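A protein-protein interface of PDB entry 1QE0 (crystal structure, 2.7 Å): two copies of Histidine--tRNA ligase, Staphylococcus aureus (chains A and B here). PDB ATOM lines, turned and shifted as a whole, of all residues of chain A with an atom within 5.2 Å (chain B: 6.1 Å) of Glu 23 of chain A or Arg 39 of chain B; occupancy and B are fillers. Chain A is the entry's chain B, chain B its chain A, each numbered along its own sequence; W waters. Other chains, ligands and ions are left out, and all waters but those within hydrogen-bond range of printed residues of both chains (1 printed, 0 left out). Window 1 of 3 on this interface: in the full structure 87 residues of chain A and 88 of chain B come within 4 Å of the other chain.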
ATOM      1  N   GLN A   9      -3.672 -11.090  -5.867  1.00  0.00           N
ATOM      2  CA  GLN A   9      -3.279 -12.384  -6.483  1.00  0.00           C
ATOM      3  C   GLN A   9      -2.674 -13.366  -5.459  1.00  0.00           C
ATOM      4  O   GLN A   9      -2.106 -12.942  -4.457  1.00  0.00           O
ATOM      5  CB  GLN A   9      -2.255 -12.168  -7.612  1.00  0.00           C
ATOM      6  CG  GLN A   9      -0.971 -11.469  -7.128  1.00  0.00           C
ATOM      7  CD  GLN A   9       0.291 -11.779  -7.945  1.00  0.00           C
ATOM      8  OE1 GLN A   9       1.409 -11.461  -7.517  1.00  0.00           O
ATOM      9  NE2 GLN A   9       0.118 -12.347  -9.131  1.00  0.00           N
ATOM     10  N   ASP A  10      -2.821 -14.665  -5.708  1.00  0.00           N
ATOM     11  CA  ASP A  10      -2.277 -15.690  -4.821  1.00  0.00           C
ATOM     12  C   ASP A  10      -0.938 -16.042  -5.392  1.00  0.00           C
ATOM     13  O   ASP A  10      -0.773 -16.032  -6.615  1.00  0.00           O
ATOM     14  CB  ASP A  10      -3.066 -16.999  -4.896  1.00  0.00           C
ATOM     15  CG  ASP A  10      -4.494 -16.861  -4.505  1.00  0.00           C
ATOM     16  OD1 ASP A  10      -4.884 -15.885  -3.846  1.00  0.00           O
ATOM     17  OD2 ASP A  10      -5.244 -17.782  -4.843  1.00  0.00           O
ATOM     18  N   ILE A  11      -0.010 -16.437  -4.533  1.00  0.00           N
ATOM     19  CA  ILE A  11       1.301 -16.864  -4.986  1.00  0.00           C
ATOM     20  C   ILE A  11       1.250 -18.385  -4.823  1.00  0.00           C
ATOM     21  O   ILE A  11       1.382 -18.897  -3.724  1.00  0.00           O
ATOM     22  CB  ILE A  11       2.398 -16.173  -4.174  1.00  0.00           C
ATOM     23  CG1 ILE A  11       2.454 -14.685  -4.582  1.00  0.00           C
ATOM     24  CG2 ILE A  11       3.709 -16.861  -4.391  1.00  0.00           C
ATOM     25  CD1 ILE A  11       3.212 -13.752  -3.622  1.00  0.00           C
ATOM     26  N   LEU A  12       0.902 -19.067  -5.919  1.00  0.00           N
ATOM     27  CA  LEU A  12       0.736 -20.526  -5.958  1.00  0.00           C
ATOM     28  C   LEU A  12       2.035 -21.308  -5.939  1.00  0.00           C
ATOM     29  O   LEU A  12       3.108 -20.751  -6.205  1.00  0.00           O
ATOM     30  CB  LEU A  12      -0.149 -20.941  -7.139  1.00  0.00           C
ATOM     31  CG  LEU A  12      -1.530 -20.265  -7.141  1.00  0.00           C
ATOM     32  CD1 LEU A  12      -2.309 -20.709  -8.336  1.00  0.00           C
ATOM     33  CD2 LEU A  12      -2.309 -20.541  -5.850  1.00  0.00           C
ATOM     34  N   SER A  16       5.810 -19.651  -5.397  1.00  0.00           N
ATOM     35  CA  SER A  16       6.219 -19.523  -3.996  1.00  0.00           C
ATOM     36  C   SER A  16       7.674 -19.885  -3.831  1.00  0.00           C
ATOM     37  O   SER A  16       8.392 -19.186  -3.148  1.00  0.00           O
ATOM     38  CB  SER A  16       5.320 -20.316  -3.040  1.00  0.00           C
ATOM     39  OG  SER A  16       5.295 -21.694  -3.335  1.00  0.00           O
ATOM     40  N   LYS A  18      10.074 -19.428  -6.058  1.00  0.00           N
ATOM     41  CA  LYS A  18      10.880 -18.347  -6.612  1.00  0.00           C
ATOM     42  C   LYS A  18      10.942 -17.240  -5.567  1.00  0.00           C
ATOM     43  O   LYS A  18      11.989 -16.592  -5.392  1.00  0.00           O
ATOM     44  CB  LYS A  18      10.245 -17.782  -7.878  1.00  0.00           C
ATOM     45  CG  LYS A  18      10.120 -18.733  -9.076  1.00  0.00           C
ATOM     46  CD  LYS A  18       9.228 -18.074 -10.158  1.00  0.00           C
ATOM     47  CE  LYS A  18       9.059 -18.911 -11.421  1.00  0.00           C
ATOM     48  NZ  LYS A  18       8.282 -20.174 -11.222  1.00  0.00           N
ATOM     49  N   TRP A  19       9.810 -16.995  -4.901  1.00  0.00           N
ATOM     50  CA  TRP A  19       9.765 -15.985  -3.854  1.00  0.00           C
ATOM     51  C   TRP A  19      10.693 -16.401  -2.733  1.00  0.00           C
ATOM     52  O   TRP A  19      11.477 -15.604  -2.269  1.00  0.00           O
ATOM     53  CB  TRP A  19       8.361 -15.817  -3.276  1.00  0.00           C
ATOM     54  CG  TRP A  19       7.475 -14.997  -4.089  1.00  0.00           C
ATOM     55  CD1 TRP A  19       6.903 -15.334  -5.270  1.00  0.00           C
ATOM     56  CD2 TRP A  19       7.104 -13.649  -3.821  1.00  0.00           C
ATOM     57  NE1 TRP A  19       6.195 -14.267  -5.771  1.00  0.00           N
ATOM     58  CE2 TRP A  19       6.291 -13.231  -4.903  1.00  0.00           C
ATOM     59  CE3 TRP A  19       7.356 -12.766  -2.780  1.00  0.00           C
ATOM     60  CZ2 TRP A  19       5.763 -11.946  -4.962  1.00  0.00           C
ATOM     61  CZ3 TRP A  19       6.831 -11.499  -2.844  1.00  0.00           C
ATOM     62  CH2 TRP A  19       6.030 -11.099  -3.924  1.00  0.00           C
ATOM     63  N   ARG A  20      10.627 -17.650  -2.301  1.00  0.00           N
ATOM     64  CA  ARG A  20      11.470 -18.072  -1.212  1.00  0.00           C
ATOM     65  C   ARG A  20      12.941 -18.020  -1.554  1.00  0.00           C
ATOM     66  O   ARG A  20      13.773 -17.761  -0.693  1.00  0.00           O
ATOM     67  CB  ARG A  20      11.094 -19.449  -0.733  1.00  0.00           C
ATOM     68  CG  ARG A  20       9.786 -19.467  -0.004  1.00  0.00           C
ATOM     69  CD  ARG A  20       9.604 -20.784   0.696  1.00  0.00           C
ATOM     70  NE  ARG A  20       9.839 -21.892  -0.223  1.00  0.00           N
ATOM     71  CZ  ARG A  20       8.892 -22.479  -0.944  1.00  0.00           C
ATOM     72  NH1 ARG A  20       9.206 -23.479  -1.754  1.00  0.00           N
ATOM     73  NH2 ARG A  20       7.630 -22.069  -0.853  1.00  0.00           N
ATOM     74  N   TYR A  21      13.279 -18.258  -2.807  1.00  0.00           N
ATOM     75  CA  TYR A  21      14.679 -18.202  -3.223  1.00  0.00           C
ATOM     76  C   TYR A  21      15.220 -16.765  -3.068  1.00  0.00           C
ATOM     77  O   TYR A  21      16.283 -16.531  -2.484  1.00  0.00           O
ATOM     78  CB  TYR A  21      14.773 -18.657  -4.669  1.00  0.00           C
ATOM     79  CG  TYR A  21      16.160 -18.631  -5.241  1.00  0.00           C
ATOM     80  CD1 TYR A  21      16.619 -17.521  -5.939  1.00  0.00           C
ATOM     81  CD2 TYR A  21      17.016 -19.710  -5.084  1.00  0.00           C
ATOM     82  CE1 TYR A  21      17.900 -17.476  -6.461  1.00  0.00           C
ATOM     83  CE2 TYR A  21      18.299 -19.689  -5.614  1.00  0.00           C
ATOM     84  CZ  TYR A  21      18.736 -18.559  -6.300  1.00  0.00           C
ATOM     85  OH  TYR A  21      20.009 -18.513  -6.826  1.00  0.00           O
ATOM     86  N   ILE A  22      14.466 -15.818  -3.608  1.00  0.00           N
ATOM     87  CA  ILE A  22      14.781 -14.397  -3.549  1.00  0.00           C
ATOM     88  C   ILE A  22      14.806 -13.933  -2.064  1.00  0.00           C
ATOM     89  O   ILE A  22      15.832 -13.477  -1.551  1.00  0.00           O
ATOM     90  CB  ILE A  22      13.738 -13.599  -4.412  1.00  0.00           C
ATOM     91  CG1 ILE A  22      14.096 -13.730  -5.892  1.00  0.00           C
ATOM     92  CG2 ILE A  22      13.669 -12.149  -3.990  1.00  0.00           C
ATOM     93  CD1 ILE A  22      12.968 -13.461  -6.842  1.00  0.00           C
ATOM     94  N   GLU A  23      13.686 -14.065  -1.377  1.00  0.00           N
ATOM     95  CA  GLU A  23      13.615 -13.715   0.008  1.00  0.00           C
ATOM     96  C   GLU A  23      14.801 -14.244   0.787  1.00  0.00           C
ATOM     97  O   GLU A  23      15.402 -13.493   1.521  1.00  0.00           O
ATOM     98  CB  GLU A  23      12.346 -14.284   0.592  1.00  0.00           C
ATOM     99  CG  GLU A  23      11.142 -13.521   0.162  1.00  0.00           C
ATOM    100  CD  GLU A  23       9.874 -14.259   0.418  1.00  0.00           C
ATOM    101  OE1 GLU A  23       9.917 -15.403   0.941  1.00  0.00           O
ATOM    102  OE2 GLU A  23       8.825 -13.694   0.067  1.00  0.00           O
ATOM    103  N   ASN A  24      15.161 -15.512   0.598  1.00  0.00           N
ATOM    104  CA  ASN A  24      16.294 -16.101   1.317  1.00  0.00           C
ATOM    105  C   ASN A  24      17.626 -15.529   0.935  1.00  0.00           C
ATOM    106  O   ASN A  24      18.504 -15.418   1.777  1.00  0.00           O
ATOM    107  CB  ASN A  24      16.371 -17.616   1.188  1.00  0.00           C
ATOM    108  CG  ASN A  24      17.606 -18.195   1.907  1.00  0.00           C
ATOM    109  OD1 ASN A  24      18.645 -18.449   1.287  1.00  0.00           O
ATOM    110  ND2 ASN A  24      17.496 -18.392   3.217  1.00  0.00           N
ATOM    111  N   GLN A  25      17.793 -15.220  -0.343  1.00  0.00           N
ATOM    112  CA  GLN A  25      19.028 -14.614  -0.836  1.00  0.00           C
ATOM    113  C   GLN A  25      19.212 -13.214  -0.240  1.00  0.00           C
ATOM    114  O   GLN A  25      20.336 -12.789   0.016  1.00  0.00           O
ATOM    115  CB  GLN A  25      18.999 -14.519  -2.366  1.00  0.00           C
ATOM    116  CG  GLN A  25      20.196 -13.794  -2.928  1.00  0.00           C
ATOM    117  CD  GLN A  25      20.754 -14.420  -4.191  1.00  0.00           C
ATOM    118  OE1 GLN A  25      20.780 -15.647  -4.344  1.00  0.00           O
ATOM    119  NE2 GLN A  25      21.219 -13.576  -5.103  1.00  0.00           N
ATOM    120  N   LEU A  26      18.108 -12.491  -0.059  1.00  0.00           N
ATOM    121  CA  LEU A  26      18.146 -11.151   0.519  1.00  0.00           C
ATOM    122  C   LEU A  26      18.519 -11.140   2.009  1.00  0.00           C
ATOM    123  O   LEU A  26      19.206 -10.239   2.462  1.00  0.00           O
ATOM    124  CB  LEU A  26      16.821 -10.450   0.301  1.00  0.00           C
ATOM    125  CG  LEU A  26      16.565  -9.998  -1.136  1.00  0.00           C
ATOM    126  CD1 LEU A  26      15.114  -9.487  -1.306  1.00  0.00           C
ATOM    127  CD2 LEU A  26      17.555  -8.919  -1.494  1.00  0.00           C
ATOM    128  N   ASP A  27      18.052 -12.116   2.774  1.00  0.00           N
ATOM    129  CA  ASP A  27      18.385 -12.205   4.183  1.00  0.00           C
ATOM    130  C   ASP A  27      19.863 -12.519   4.331  1.00  0.00           C
ATOM    131  O   ASP A  27      20.503 -12.130   5.300  1.00  0.00           O
ATOM    132  CB  ASP A  27      17.599 -13.317   4.851  1.00  0.00           C
ATOM    133  CG  ASP A  27      16.110 -13.136   4.721  1.00  0.00           C
ATOM    134  OD1 ASP A  27      15.659 -11.960   4.608  1.00  0.00           O
ATOM    135  OD2 ASP A  27      15.403 -14.181   4.729  1.00  0.00           O
ATOM    136  N   ASN A 107      10.649  -6.913   4.726  1.00  0.00           N
ATOM    137  CA  ASN A 107      10.197  -7.551   3.522  1.00  0.00           C
ATOM    138  C   ASN A 107       8.805  -8.039   3.814  1.00  0.00           C
ATOM    139  O   ASN A 107       8.643  -8.883   4.674  1.00  0.00           O
ATOM    140  CB  ASN A 107      11.106  -8.716   3.204  1.00  0.00           C
ATOM    141  CG  ASN A 107      10.761  -9.353   1.882  1.00  0.00           C
ATOM    142  OD1 ASN A 107       9.666  -9.121   1.355  1.00  0.00           O
ATOM    143  ND2 ASN A 107      11.712 -10.102   1.290  1.00  0.00           N
ATOM    144  N   GLU B  37       4.208 -24.398  -1.036  1.00  0.00           N
ATOM    145  CA  GLU B  37       3.735 -23.170  -0.401  1.00  0.00           C
ATOM    146  C   GLU B  37       2.808 -22.317  -1.225  1.00  0.00           C
ATOM    147  O   GLU B  37       3.054 -22.090  -2.391  1.00  0.00           O
ATOM    148  CB  GLU B  37       4.891 -22.287   0.036  1.00  0.00           C
ATOM    149  CG  GLU B  37       4.403 -21.143   0.916  1.00  0.00           C
ATOM    150  CD  GLU B  37       5.459 -20.107   1.239  1.00  0.00           C
ATOM    151  OE1 GLU B  37       6.434 -19.945   0.483  1.00  0.00           O
ATOM    152  OE2 GLU B  37       5.289 -19.412   2.247  1.00  0.00           O
ATOM    153  N   ILE B  38       1.753 -21.815  -0.603  1.00  0.00           N
ATOM    154  CA  ILE B  38       0.815 -20.962  -1.298  1.00  0.00           C
ATOM    155  C   ILE B  38       0.693 -19.741  -0.386  1.00  0.00           C
ATOM    156  O   ILE B  38       0.823 -19.861   0.829  1.00  0.00           O
ATOM    157  CB  ILE B  38      -0.550 -21.678  -1.487  1.00  0.00           C
ATOM    158  CG1 ILE B  38      -1.536 -20.820  -2.289  1.00  0.00           C
ATOM    159  CG2 ILE B  38      -1.165 -22.034  -0.134  1.00  0.00           C
ATOM    160  CD1 ILE B  38      -2.896 -21.478  -2.411  1.00  0.00           C
ATOM    161  N   ARG B  39       0.538 -18.562  -0.976  1.00  0.00           N
ATOM    162  CA  ARG B  39       0.423 -17.326  -0.236  1.00  0.00           C
ATOM    163  C   ARG B  39      -0.805 -16.620  -0.737  1.00  0.00           C
ATOM    164  O   ARG B  39      -0.871 -16.172  -1.864  1.00  0.00           O
ATOM    165  CB  ARG B  39       1.626 -16.451  -0.487  1.00  0.00           C
ATOM    166  CG  ARG B  39       2.927 -17.180  -0.437  1.00  0.00           C
ATOM    167  CD  ARG B  39       4.047 -16.249  -0.086  1.00  0.00           C
ATOM    168  NE  ARG B  39       5.275 -16.992   0.100  1.00  0.00           N
ATOM    169  CZ  ARG B  39       6.462 -16.424   0.082  1.00  0.00           C
ATOM    170  NH1 ARG B  39       6.536 -15.122  -0.105  1.00  0.00           N
ATOM    171  NH2 ARG B  39       7.566 -17.148   0.200  1.00  0.00           N
ATOM    172  N   THR B  40      -1.795 -16.563   0.120  1.00  0.00           N
ATOM    173  CA  THR B  40      -3.091 -15.965  -0.137  1.00  0.00           C
ATOM    174  C   THR B  40      -3.016 -14.494   0.311  1.00  0.00           C
ATOM    175  O   THR B  40      -2.112 -14.116   1.053  1.00  0.00           O
ATOM    176  CB  THR B  40      -4.068 -16.782   0.749  1.00  0.00           C
ATOM    177  OG1 THR B  40      -4.461 -17.941   0.028  1.00  0.00           O
ATOM    178  CG2 THR B  40      -5.254 -15.978   1.297  1.00  0.00           C
ATOM    179  N   PRO B  41      -3.905 -13.632  -0.187  1.00  0.00           N
ATOM    180  CA  PRO B  41      -3.899 -12.215   0.213  1.00  0.00           C
ATOM    181  C   PRO B  41      -4.211 -12.057   1.706  1.00  0.00           C
ATOM    182  O   PRO B  41      -4.796 -12.951   2.340  1.00  0.00           O
ATOM    183  CB  PRO B  41      -5.022 -11.626  -0.632  1.00  0.00           C
ATOM    184  CG  PRO B  41      -4.957 -12.484  -1.853  1.00  0.00           C
ATOM    185  CD  PRO B  41      -4.820 -13.858  -1.308  1.00  0.00           C
ATOM    186  N   ARG B  78      -8.231 -11.948   6.907  1.00  0.00           N
ATOM    187  CA  ARG B  78      -8.366 -13.368   7.187  1.00  0.00           C
ATOM    188  C   ARG B  78      -8.048 -13.734   8.645  1.00  0.00           C
ATOM    189  O   ARG B  78      -7.120 -13.196   9.242  1.00  0.00           O
ATOM    190  CB  ARG B  78      -7.453 -14.162   6.273  1.00  0.00           C
ATOM    191  CG  ARG B  78      -6.052 -13.900   6.568  1.00  0.00           C
ATOM    192  CD  ARG B  78      -5.169 -14.637   5.638  1.00  0.00           C
ATOM    193  NE  ARG B  78      -3.788 -14.561   6.079  1.00  0.00           N
ATOM    194  CZ  ARG B  78      -2.750 -14.369   5.269  1.00  0.00           C
ATOM    195  NH1 ARG B  78      -2.938 -14.227   3.974  1.00  0.00           N
ATOM    196  NH2 ARG B  78      -1.512 -14.343   5.742  1.00  0.00           N
ATOM    197  N   TYR B 105       0.930 -25.904   1.842  1.00  0.00           N
ATOM    198  CA  TYR B 105       1.194 -25.349   3.164  1.00  0.00           C
ATOM    199  C   TYR B 105       1.292 -23.844   3.101  1.00  0.00           C
ATOM    200  O   TYR B 105       1.489 -23.264   2.022  1.00  0.00           O
ATOM    201  CB  TYR B 105       2.465 -25.926   3.796  1.00  0.00           C
ATOM    202  CG  TYR B 105       3.789 -25.295   3.412  1.00  0.00           C
ATOM    203  CD1 TYR B 105       4.307 -24.204   4.095  1.00  0.00           C
ATOM    204  CD2 TYR B 105       4.552 -25.845   2.408  1.00  0.00           C
ATOM    205  CE1 TYR B 105       5.550 -23.695   3.783  1.00  0.00           C
ATOM    206  CE2 TYR B 105       5.793 -25.340   2.079  1.00  0.00           C
ATOM    207  CZ  TYR B 105       6.289 -24.281   2.760  1.00  0.00           C
ATOM    208  OH  TYR B 105       7.542 -23.838   2.394  1.00  0.00           O
ATOM    209  N   TYR B 106       1.107 -23.197   4.247  1.00  0.00           N
ATOM    210  CA  TYR B 106       1.175 -21.745   4.302  1.00  0.00           C
ATOM    211  C   TYR B 106       1.808 -21.324   5.593  1.00  0.00           C
ATOM    212  O   TYR B 106       2.065 -22.152   6.452  1.00  0.00           O
ATOM    213  CB  TYR B 106      -0.208 -21.136   4.149  1.00  0.00           C
ATOM    214  CG  TYR B 106      -1.185 -21.553   5.187  1.00  0.00           C
ATOM    215  CD1 TYR B 106      -2.178 -22.485   4.897  1.00  0.00           C
ATOM    216  CD2 TYR B 106      -1.113 -21.039   6.475  1.00  0.00           C
ATOM    217  CE1 TYR B 106      -3.071 -22.902   5.874  1.00  0.00           C
ATOM    218  CE2 TYR B 106      -2.002 -21.449   7.465  1.00  0.00           C
ATOM    219  CZ  TYR B 106      -2.971 -22.379   7.163  1.00  0.00           C
ATOM    220  OH  TYR B 106      -3.812 -22.800   8.161  1.00  0.00           O
HETATM  221  O   HOH W   1       6.793 -24.621  -2.275  1.00  0.00           O
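OG of Ser 16 of chain A is in hydrogen-bond range of O of Glu 37 of chain B.
NH2 of Arg 20 of chain A is in salt-bridge range of OE1 of Glu 37 of chain B (2.8 Å).
The backbone carbonyl oxygen (O) of Arg 39 of chain B is in hydrogen-bond range of the backbone NH (N) of Ile 11 of chain A (2.8 Å).
NH1 of Arg 39 of chain B is in salt-bridge range of OE2 of Glu 23 of chain A, 2.7 Å away.
OE1 of Glu 37 of chain B lies within salt-bridge range of NH2 of Arg 39 of chain B (3.0 Å).
The backbone carbonyl oxygen (O) of Tyr 105 of chain B lies within hydrogen-bond range of the backbone NH (N) of Ile 38 of chain B (3.0 Å).
The backbone carbonyl oxygen (O) of Pro 41 of chain B sits at hydrogen-bond distance from the guanidinium group (NH1) of Arg 78 of chain B (2.8 Å).
OG of Ser 16 of chain A sits at hydrogen-bond distance from NH2 of Arg 20 of chain A.
Among the printed residues, pairs that only touch across the chains: Gln 9 of chain A with Pro 41 of chain B (3.9 Å), Asp 10 of chain A with Arg 39 of chain B (3.3 Å), Asp 10 of chain A with Pro 41 of chain B (3.2 Å), Ile 11 of chain A with Glu 37 of chain B (3.8 Å), Ile 11 of chain A with Ile 38 of chain B (3.2 Å), Leu 12 of chain A with Glu 37 of chain B (3.8 Å), Leu 12 of chain A with Ile 38 of chain B (3.6 Å), Trp 19 of chain A with Arg 39 of chain B (3.7 Å), Arg 20 of chain A with Arg 39 of chain B (3.2 Å) and Arg 20 of chain A with Tyr 105 of chain B (3.7 Å).
Printed residues of chain B within 4 Å of Leu 12 of chain A: Glu 37 (3.8 Å) and Ile 38 (3.6 Å).
Of the printed residues of chain B, Glu 23 of chain A touches Arg 39.
Asn 24 of chain A touches none of the printed residues of chain B.
Of the printed residues of chain A, Ile 38 of chain B touches Ile 11 and Leu 12.
Of the printed residues of chain A, Arg 39 of chain B touches Asp 10, Ile 11, Trp 19, Arg 20 and Glu 23.
Of the printed residues of chain A, Tyr 105 of chain B touches Arg 20 (3.7 Å).
The nearest printed residue of chain A that does not touch Pro 41 of chain B is Ile 11 of chain A (6.3 Å).
Of the 16 printed residues of chain A, 8 touch a printed residue of chain B.
Hydrophobic or aromatic side chains of chain A that line the printed part of chain B: Ile 11, Leu 12 and Trp 19.
Of the 8 printed residues of chain B, 5 touch a printed residue of chain A.
Hydrophobic or aromatic side chains of chain B within 4 Å of the printed part of chain A: Ile 38, Pro 41 and Tyr 105.
No position is printed for both chains.
Of the 14 pairs that touch across the chains among the printed residues, none has its exchanged pair printed and touching as well.
Water W1 lies within hydrogen-bond range of the guanidinium group of Arg 20 of chain A, the backbone NH of Glu 37 of chain B and the side-chain hydroxyl of Ser 16 of chain A.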
